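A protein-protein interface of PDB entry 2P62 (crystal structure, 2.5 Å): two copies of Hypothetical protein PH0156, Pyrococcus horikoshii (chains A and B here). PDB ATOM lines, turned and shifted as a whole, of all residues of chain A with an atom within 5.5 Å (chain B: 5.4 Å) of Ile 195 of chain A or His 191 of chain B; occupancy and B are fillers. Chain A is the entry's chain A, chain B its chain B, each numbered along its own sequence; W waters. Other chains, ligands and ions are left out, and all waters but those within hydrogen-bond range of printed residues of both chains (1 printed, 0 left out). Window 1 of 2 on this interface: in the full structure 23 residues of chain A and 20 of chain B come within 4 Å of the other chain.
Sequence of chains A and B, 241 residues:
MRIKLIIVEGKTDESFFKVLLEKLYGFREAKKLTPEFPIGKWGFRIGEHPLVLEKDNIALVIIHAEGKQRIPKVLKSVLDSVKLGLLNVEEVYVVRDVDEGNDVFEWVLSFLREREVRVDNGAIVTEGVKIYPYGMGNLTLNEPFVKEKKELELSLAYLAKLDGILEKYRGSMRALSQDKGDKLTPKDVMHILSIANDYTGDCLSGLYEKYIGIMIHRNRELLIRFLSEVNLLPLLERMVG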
ATOM      1  N   TYR A 169      -0.810 -16.121  32.350  1.00  0.00           N
ATOM      2  CA  TYR A 169       0.443 -15.590  31.856  1.00  0.00           C
ATOM      3  C   TYR A 169       0.279 -14.102  31.573  1.00  0.00           C
ATOM      4  O   TYR A 169       0.148 -13.312  32.505  1.00  0.00           O
ATOM      5  CB  TYR A 169       0.915 -16.388  30.620  1.00  0.00           C
ATOM      6  CG  TYR A 169       1.545 -17.720  31.014  1.00  0.00           C
ATOM      7  CD1 TYR A 169       0.771 -18.742  31.574  1.00  0.00           C
ATOM      8  CD2 TYR A 169       2.935 -17.890  30.997  1.00  0.00           C
ATOM      9  CE1 TYR A 169       1.362 -19.888  32.130  1.00  0.00           C
ATOM     10  CE2 TYR A 169       3.540 -19.033  31.550  1.00  0.00           C
ATOM     11  CZ  TYR A 169       2.748 -20.024  32.124  1.00  0.00           C
ATOM     12  OH  TYR A 169       3.331 -21.105  32.762  1.00  0.00           O
ATOM     13  N   HIS A 191       3.926 -21.659  21.633  1.00  0.00           N
ATOM     14  CA  HIS A 191       5.110 -22.058  22.369  1.00  0.00           C
ATOM     15  C   HIS A 191       5.015 -21.703  23.843  1.00  0.00           C
ATOM     16  O   HIS A 191       5.640 -22.353  24.678  1.00  0.00           O
ATOM     17  CB  HIS A 191       6.359 -21.446  21.745  1.00  0.00           C
ATOM     18  CG  HIS A 191       6.756 -22.104  20.466  1.00  0.00           C
ATOM     19  ND1 HIS A 191       6.469 -21.566  19.230  1.00  0.00           N
ATOM     20  CD2 HIS A 191       7.349 -23.297  20.229  1.00  0.00           C
ATOM     21  CE1 HIS A 191       6.866 -22.400  18.287  1.00  0.00           C
ATOM     22  NE2 HIS A 191       7.403 -23.460  18.866  1.00  0.00           N
ATOM     23  N   ILE A 192       4.236 -20.674  24.166  1.00  0.00           N
ATOM     24  CA  ILE A 192       4.056 -20.290  25.556  1.00  0.00           C
ATOM     25  C   ILE A 192       3.187 -21.374  26.164  1.00  0.00           C
ATOM     26  O   ILE A 192       3.369 -21.755  27.322  1.00  0.00           O
ATOM     27  CB  ILE A 192       3.338 -18.940  25.679  1.00  0.00           C
ATOM     28  CG1 ILE A 192       4.220 -17.843  25.093  1.00  0.00           C
ATOM     29  CG2 ILE A 192       2.987 -18.663  27.142  1.00  0.00           C
ATOM     30  CD1 ILE A 192       3.626 -16.476  25.198  1.00  0.00           C
ATOM     31  N   LEU A 193       2.244 -21.873  25.366  1.00  0.00           N
ATOM     32  CA  LEU A 193       1.348 -22.940  25.801  1.00  0.00           C
ATOM     33  C   LEU A 193       2.158 -24.200  26.142  1.00  0.00           C
ATOM     34  O   LEU A 193       1.829 -24.904  27.090  1.00  0.00           O
ATOM     35  CB  LEU A 193       0.318 -23.269  24.708  1.00  0.00           C
ATOM     36  CG  LEU A 193      -0.668 -24.413  25.006  1.00  0.00           C
ATOM     37  CD1 LEU A 193      -1.574 -24.023  26.167  1.00  0.00           C
ATOM     38  CD2 LEU A 193      -1.518 -24.721  23.775  1.00  0.00           C
ATOM     39  N   SER A 194       3.212 -24.486  25.376  1.00  0.00           N
ATOM     40  CA  SER A 194       4.043 -25.660  25.642  1.00  0.00           C
ATOM     41  C   SER A 194       4.672 -25.545  27.031  1.00  0.00           C
ATOM     42  O   SER A 194       4.786 -26.527  27.772  1.00  0.00           O
ATOM     43  CB  SER A 194       5.163 -25.790  24.603  1.00  0.00           C
ATOM     44  OG  SER A 194       4.663 -26.020  23.306  1.00  0.00           O
ATOM     45  N   ILE A 195       5.090 -24.332  27.365  1.00  0.00           N
ATOM     46  CA  ILE A 195       5.707 -24.056  28.650  1.00  0.00           C
ATOM     47  C   ILE A 195       4.664 -24.105  29.759  1.00  0.00           C
ATOM     48  O   ILE A 195       4.903 -24.680  30.823  1.00  0.00           O
ATOM     49  CB  ILE A 195       6.361 -22.672  28.636  1.00  0.00           C
ATOM     50  CG1 ILE A 195       7.466 -22.647  27.574  1.00  0.00           C
ATOM     51  CG2 ILE A 195       6.866 -22.323  30.024  1.00  0.00           C
ATOM     52  CD1 ILE A 195       8.074 -21.272  27.336  1.00  0.00           C
ATOM     53  N   ALA A 196       3.501 -23.513  29.504  1.00  0.00           N
ATOM     54  CA  ALA A 196       2.433 -23.489  30.496  1.00  0.00           C
ATOM     55  C   ALA A 196       1.909 -24.879  30.816  1.00  0.00           C
ATOM     56  O   ALA A 196       1.372 -25.102  31.896  1.00  0.00           O
ATOM     57  CB  ALA A 196       1.289 -22.603  30.017  1.00  0.00           C
ATOM     58  N   ASN A 197       2.053 -25.816  29.883  1.00  0.00           N
ATOM     59  CA  ASN A 197       1.569 -27.174  30.128  1.00  0.00           C
ATOM     60  C   ASN A 197       2.726 -28.134  30.345  1.00  0.00           C
ATOM     61  O   ASN A 197       2.532 -29.345  30.444  1.00  0.00           O
ATOM     62  CB  ASN A 197       0.716 -27.669  28.959  1.00  0.00           C
ATOM     63  CG  ASN A 197      -0.535 -26.838  28.755  1.00  0.00           C
ATOM     64  OD1 ASN A 197      -1.377 -27.162  27.921  1.00  0.00           O
ATOM     65  ND2 ASN A 197      -0.660 -25.757  29.516  1.00  0.00           N
ATOM     66  N   ASP A 198       3.929 -27.580  30.437  1.00  0.00           N
ATOM     67  CA  ASP A 198       5.133 -28.378  30.632  1.00  0.00           C
ATOM     68  C   ASP A 198       5.190 -29.500  29.593  1.00  0.00           C
ATOM     69  O   ASP A 198       5.369 -30.673  29.933  1.00  0.00           O
ATOM     70  CB  ASP A 198       5.157 -28.976  32.045  1.00  0.00           C
ATOM     71  CG  ASP A 198       6.550 -29.476  32.447  1.00  0.00           C
ATOM     72  OD1 ASP A 198       6.637 -30.428  33.256  1.00  0.00           O
ATOM     73  OD2 ASP A 198       7.555 -28.906  31.964  1.00  0.00           O
ATOM     74  N   TYR A 199       5.025 -29.131  28.324  1.00  0.00           N
ATOM     75  CA  TYR A 199       5.065 -30.090  27.223  1.00  0.00           C
ATOM     76  C   TYR A 199       6.507 -30.417  26.899  1.00  0.00           C
ATOM     77  O   TYR A 199       7.287 -29.527  26.582  1.00  0.00           O
ATOM     78  CB  TYR A 199       4.414 -29.509  25.978  1.00  0.00           C
ATOM     79  CG  TYR A 199       4.385 -30.473  24.818  1.00  0.00           C
ATOM     80  CD1 TYR A 199       3.695 -31.683  24.913  1.00  0.00           C
ATOM     81  CD2 TYR A 199       5.041 -30.179  23.626  1.00  0.00           C
ATOM     82  CE1 TYR A 199       3.659 -32.573  23.845  1.00  0.00           C
ATOM     83  CE2 TYR A 199       5.011 -31.060  22.558  1.00  0.00           C
ATOM     84  CZ  TYR A 199       4.320 -32.253  22.672  1.00  0.00           C
ATOM     85  OH  TYR A 199       4.287 -33.131  21.612  1.00  0.00           O
ATOM     86  N   GLY A 201       7.315 -32.914  24.562  1.00  0.00           N
ATOM     87  CA  GLY A 201       7.430 -33.485  23.232  1.00  0.00           C
ATOM     88  C   GLY A 201       8.158 -32.611  22.237  1.00  0.00           C
ATOM     89  O   GLY A 201       8.443 -31.447  22.505  1.00  0.00           O
ATOM     90  N   LEU A 204       4.530 -29.598  18.216  1.00  0.00           N
ATOM     91  CA  LEU A 204       3.376 -28.901  18.742  1.00  0.00           C
ATOM     92  C   LEU A 204       2.119 -29.704  18.414  1.00  0.00           C
ATOM     93  O   LEU A 204       1.148 -29.689  19.171  1.00  0.00           O
ATOM     94  CB  LEU A 204       3.286 -27.505  18.126  1.00  0.00           C
ATOM     95  CG  LEU A 204       4.399 -26.526  18.507  1.00  0.00           C
ATOM     96  CD1 LEU A 204       4.259 -25.278  17.662  1.00  0.00           C
ATOM     97  CD2 LEU A 204       4.335 -26.189  20.000  1.00  0.00           C
ATOM     98  N   LEU B 176       8.386 -15.678  32.488  1.00  0.00           N
ATOM     99  CA  LEU B 176       7.861 -17.034  32.316  1.00  0.00           C
ATOM    100  C   LEU B 176       8.018 -17.855  33.589  1.00  0.00           C
ATOM    101  O   LEU B 176       7.127 -18.624  33.957  1.00  0.00           O
ATOM    102  CB  LEU B 176       8.560 -17.771  31.164  1.00  0.00           C
ATOM    103  CG  LEU B 176       7.965 -17.726  29.748  1.00  0.00           C
ATOM    104  CD1 LEU B 176       6.500 -18.169  29.765  1.00  0.00           C
ATOM    105  CD2 LEU B 176       8.074 -16.336  29.202  1.00  0.00           C
ATOM    106  N   LYS B 180       5.049 -19.455  35.677  1.00  0.00           N
ATOM    107  CA  LYS B 180       5.061 -20.906  35.790  1.00  0.00           C
ATOM    108  C   LYS B 180       5.108 -21.300  37.263  1.00  0.00           C
ATOM    109  O   LYS B 180       4.669 -22.388  37.640  1.00  0.00           O
ATOM    110  CB  LYS B 180       6.267 -21.484  35.047  1.00  0.00           C
ATOM    111  CG  LYS B 180       6.237 -22.998  34.858  1.00  0.00           C
ATOM    112  CD  LYS B 180       7.545 -23.473  34.225  1.00  0.00           C
ATOM    113  CE  LYS B 180       7.594 -24.984  33.995  1.00  0.00           C
ATOM    114  NZ  LYS B 180       6.639 -25.466  32.948  1.00  0.00           N
ATOM    115  N   LEU B 184      12.503 -22.465  34.886  1.00  0.00           N
ATOM    116  CA  LEU B 184      12.278 -23.012  33.558  1.00  0.00           C
ATOM    117  C   LEU B 184      13.181 -24.212  33.291  1.00  0.00           C
ATOM    118  O   LEU B 184      14.300 -24.291  33.806  1.00  0.00           O
ATOM    119  CB  LEU B 184      12.553 -21.937  32.504  1.00  0.00           C
ATOM    120  CG  LEU B 184      11.684 -20.683  32.557  1.00  0.00           C
ATOM    121  CD1 LEU B 184      12.123 -19.719  31.468  1.00  0.00           C
ATOM    122  CD2 LEU B 184      10.226 -21.054  32.376  1.00  0.00           C
ATOM    123  N   LYS B 187      14.072 -27.448  28.249  1.00  0.00           N
ATOM    124  CA  LYS B 187      13.105 -27.654  27.184  1.00  0.00           C
ATOM    125  C   LYS B 187      12.218 -26.414  27.030  1.00  0.00           C
ATOM    126  O   LYS B 187      11.858 -26.059  25.909  1.00  0.00           O
ATOM    127  CB  LYS B 187      12.260 -28.902  27.444  1.00  0.00           C
ATOM    128  CG  LYS B 187      12.962 -30.200  27.048  1.00  0.00           C
ATOM    129  CD  LYS B 187      11.961 -31.327  26.847  1.00  0.00           C
ATOM    130  CE  LYS B 187      12.623 -32.592  26.295  1.00  0.00           C
ATOM    131  NZ  LYS B 187      13.600 -33.192  27.260  1.00  0.00           N
ATOM    132  N   ASP B 188      11.870 -25.749  28.135  1.00  0.00           N
ATOM    133  CA  ASP B 188      11.060 -24.529  28.039  1.00  0.00           C
ATOM    134  C   ASP B 188      11.852 -23.464  27.266  1.00  0.00           C
ATOM    135  O   ASP B 188      11.278 -22.709  26.483  1.00  0.00           O
ATOM    136  CB  ASP B 188      10.703 -23.941  29.421  1.00  0.00           C
ATOM    137  CG  ASP B 188       9.801 -24.845  30.251  1.00  0.00           C
ATOM    138  OD1 ASP B 188       8.867 -25.465  29.699  1.00  0.00           O
ATOM    139  OD2 ASP B 188      10.017 -24.913  31.483  1.00  0.00           O
ATOM    140  N   VAL B 189      13.165 -23.397  27.497  1.00  0.00           N
ATOM    141  CA  VAL B 189      14.005 -22.408  26.814  1.00  0.00           C
ATOM    142  C   VAL B 189      13.988 -22.659  25.310  1.00  0.00           C
ATOM    143  O   VAL B 189      14.094 -21.737  24.494  1.00  0.00           O
ATOM    144  CB  VAL B 189      15.471 -22.461  27.319  1.00  0.00           C
ATOM    145  CG1 VAL B 189      16.353 -21.525  26.482  1.00  0.00           C
ATOM    146  CG2 VAL B 189      15.529 -22.065  28.797  1.00  0.00           C
ATOM    147  N   MET B 190      13.853 -23.926  24.952  1.00  0.00           N
ATOM    148  CA  MET B 190      13.806 -24.304  23.556  1.00  0.00           C
ATOM    149  C   MET B 190      12.555 -23.656  22.963  1.00  0.00           C
ATOM    150  O   MET B 190      12.534 -23.284  21.788  1.00  0.00           O
ATOM    151  CB  MET B 190      13.748 -25.826  23.443  1.00  0.00           C
ATOM    152  CG  MET B 190      14.872 -26.455  22.634  1.00  0.00           C
ATOM    153  SD  MET B 190      16.562 -26.088  23.092  1.00  0.00           S
ATOM    154  CE  MET B 190      17.099 -25.316  21.735  1.00  0.00           C
ATOM    155  N   HIS B 191      11.513 -23.487  23.771  1.00  0.00           N
ATOM    156  CA  HIS B 191      10.310 -22.863  23.235  1.00  0.00           C
ATOM    157  C   HIS B 191      10.438 -21.344  23.120  1.00  0.00           C
ATOM    158  O   HIS B 191       9.763 -20.713  22.304  1.00  0.00           O
ATOM    159  CB  HIS B 191       9.084 -23.287  24.044  1.00  0.00           C
ATOM    160  CG  HIS B 191       8.709 -24.722  23.822  1.00  0.00           C
ATOM    161  ND1 HIS B 191       8.235 -25.188  22.612  1.00  0.00           N
ATOM    162  CD2 HIS B 191       8.801 -25.804  24.629  1.00  0.00           C
ATOM    163  CE1 HIS B 191       8.053 -26.494  22.686  1.00  0.00           C
ATOM    164  NE2 HIS B 191       8.389 -26.894  23.898  1.00  0.00           N
ATOM    165  N   ILE B 192      11.339 -20.769  23.909  1.00  0.00           N
ATOM    166  CA  ILE B 192      11.604 -19.334  23.871  1.00  0.00           C
ATOM    167  C   ILE B 192      12.428 -19.069  22.615  1.00  0.00           C
ATOM    168  O   ILE B 192      12.263 -18.058  21.939  1.00  0.00           O
ATOM    169  CB  ILE B 192      12.427 -18.882  25.104  1.00  0.00           C
ATOM    170  CG1 ILE B 192      11.544 -18.892  26.347  1.00  0.00           C
ATOM    171  CG2 ILE B 192      13.048 -17.503  24.857  1.00  0.00           C
ATOM    172  CD1 ILE B 192      12.321 -18.773  27.650  1.00  0.00           C
ATOM    173  N   LEU B 193      13.330 -19.994  22.316  1.00  0.00           N
ATOM    174  CA  LEU B 193      14.169 -19.860  21.143  1.00  0.00           C
ATOM    175  C   LEU B 193      13.307 -19.825  19.873  1.00  0.00           C
ATOM    176  O   LEU B 193      13.613 -19.099  18.919  1.00  0.00           O
ATOM    177  CB  LEU B 193      15.152 -21.023  21.093  1.00  0.00           C
ATOM    178  CG  LEU B 193      16.131 -21.042  19.928  1.00  0.00           C
ATOM    179  CD1 LEU B 193      17.054 -19.831  19.971  1.00  0.00           C
ATOM    180  CD2 LEU B 193      16.919 -22.338  20.002  1.00  0.00           C
ATOM    181  N   SER B 194      12.227 -20.603  19.871  1.00  0.00           N
ATOM    182  CA  SER B 194      11.310 -20.668  18.732  1.00  0.00           C
ATOM    183  C   SER B 194      10.735 -19.289  18.452  1.00  0.00           C
ATOM    184  O   SER B 194      10.668 -18.843  17.305  1.00  0.00           O
ATOM    185  CB  SER B 194      10.164 -21.639  19.021  1.00  0.00           C
ATOM    186  OG  SER B 194      10.649 -22.954  19.253  1.00  0.00           O
ATOM    187  N   ILE B 195      10.311 -18.619  19.516  1.00  0.00           N
ATOM    188  CA  ILE B 195       9.750 -17.287  19.394  1.00  0.00           C
ATOM    189  C   ILE B 195      10.840 -16.304  18.975  1.00  0.00           C
ATOM    190  O   ILE B 195      10.629 -15.488  18.082  1.00  0.00           O
ATOM    191  CB  ILE B 195       9.130 -16.831  20.727  1.00  0.00           C
ATOM    192  CG1 ILE B 195       8.121 -17.883  21.204  1.00  0.00           C
ATOM    193  CG2 ILE B 195       8.455 -15.480  20.548  1.00  0.00           C
ATOM    194  CD1 ILE B 195       7.499 -17.604  22.555  1.00  0.00           C
ATOM    195  N   LEU B 204      10.461 -29.040  17.190  1.00  0.00           N
ATOM    196  CA  LEU B 204      11.694 -28.425  17.678  1.00  0.00           C
ATOM    197  C   LEU B 204      12.888 -29.023  16.937  1.00  0.00           C
ATOM    198  O   LEU B 204      13.891 -28.341  16.685  1.00  0.00           O
ATOM    199  CB  LEU B 204      11.839 -28.654  19.188  1.00  0.00           C
ATOM    200  CG  LEU B 204      10.741 -27.992  20.029  1.00  0.00           C
ATOM    201  CD1 LEU B 204      10.802 -28.464  21.472  1.00  0.00           C
ATOM    202  CD2 LEU B 204      10.899 -26.489  19.945  1.00  0.00           C
HETATM  203  O   HOH W   1       8.861 -29.509  24.493  1.00  0.00           O
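Of chain B, only Lys 180, Asp 188 and His 191 come within 4 Å of Ile 195 of chain A.
His 191 of chain B touches just these residues of chain A: His 191 (3.2 Å), Ser 194 (3.5 Å), Ile 195 (3.9 Å) and Tyr 199 (3.9 Å).
Of the printed residues of chain B, His 191 of chain A touches His 191 (3.2 Å) and Ser 194 (3.3 Å).
Of the printed residues of chain B, Tyr 199 of chain A touches His 191 (3.9 Å).
The nearest residue of chain A that does not touch His 191 of chain B is Leu 204 of chain A (4.6 Å).
His 191 of chain B touches its own counterpart, His 191 of chain A.
His 191 of chain A touches Ser 194 of chain B, and with the chains exchanged Ser 194 of chain A touches His 191 of chain B.
Ile 195 of chain A touches His 191 of chain B, but with the chains exchanged His 191 of chain A does not touch Ile 195 of chain B (4.01 Å).
Of the 12 printed residues of chain A, 7 touch a printed residue of chain B.
Printed residues of chain A that touch a printed residue of chain B: Tyr 169, His 191, Ser 194, Ile 195, Asp 198, Tyr 199 and Gly 201.
Hydrophobic or aromatic side chains of chain A that line the printed part of chain B: Tyr 169, His 191 and Ile 195.
Hydrophobic or aromatic side chains of chain B that line the printed part of chain A: Leu 176, His 191 and Leu 204.
Among the printed residues, Asp or Glu carboxylates within 4 Å of a Lys or Arg side-chain nitrogen of the other chain: Asp 198 of chain A with Lys 180 of chain B (3.7 Å).
CE2 of Tyr 169 of chain A touches CD1 of Leu 176 of chain B, at 3.6 Å.
Lys 180 of chain B touches Tyr 169 of chain A.
His 191 of chain B touches His 191 of chain A (ND1 to CD2, 3.2 Å).
Ser 194 of chain A touches His 191 of chain B.
Ile 195 of chain A touches Asp 188 of chain B.
His 191 of chain B touches Ile 195 of chain A.
His 191 of chain B touches Tyr 199 of chain A (NE2 to O, 3.9 Å).
Gly 201 of chain A touches Leu 204 of chain B.
The backbone carbonyl oxygen (O) of Ser 194 of chain A lies within hydrogen-bond range of the backbone NH (N) of Tyr 199 of chain A (2.7 Å).
The side-chain amino group of Lys 180 of chain B is in salt-bridge range of the side-chain carboxylate of Asp 188 of chain B, at 3.7 Å.
The backbone carbonyl oxygen of Met 190 of chain B lies within hydrogen-bond range of the side-chain hydroxyl of Ser 194 of chain B (3.2 Å).
Water W1 lies within hydrogen-bond range of O of Tyr 199 of chain A (2.6 Å), NE2 of His 191 of chain B (2.7 Å) and O of Gly 201 of chain A (2.8 Å).
A ring nitrogen (NE2) of His 191 of chain A sits at hydrogen-bond distance from the side-chain hydroxyl of Ser 194 of chain B (3.3 Å).
O of Ile 195 of chain A lies within hydrogen-bond range of NZ of Lys 180 of chain B (2.9 Å).
NZ of Lys 180 of chain B lies within salt-bridge range of OD2 of Asp 198 of chain A (3.7 Å).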
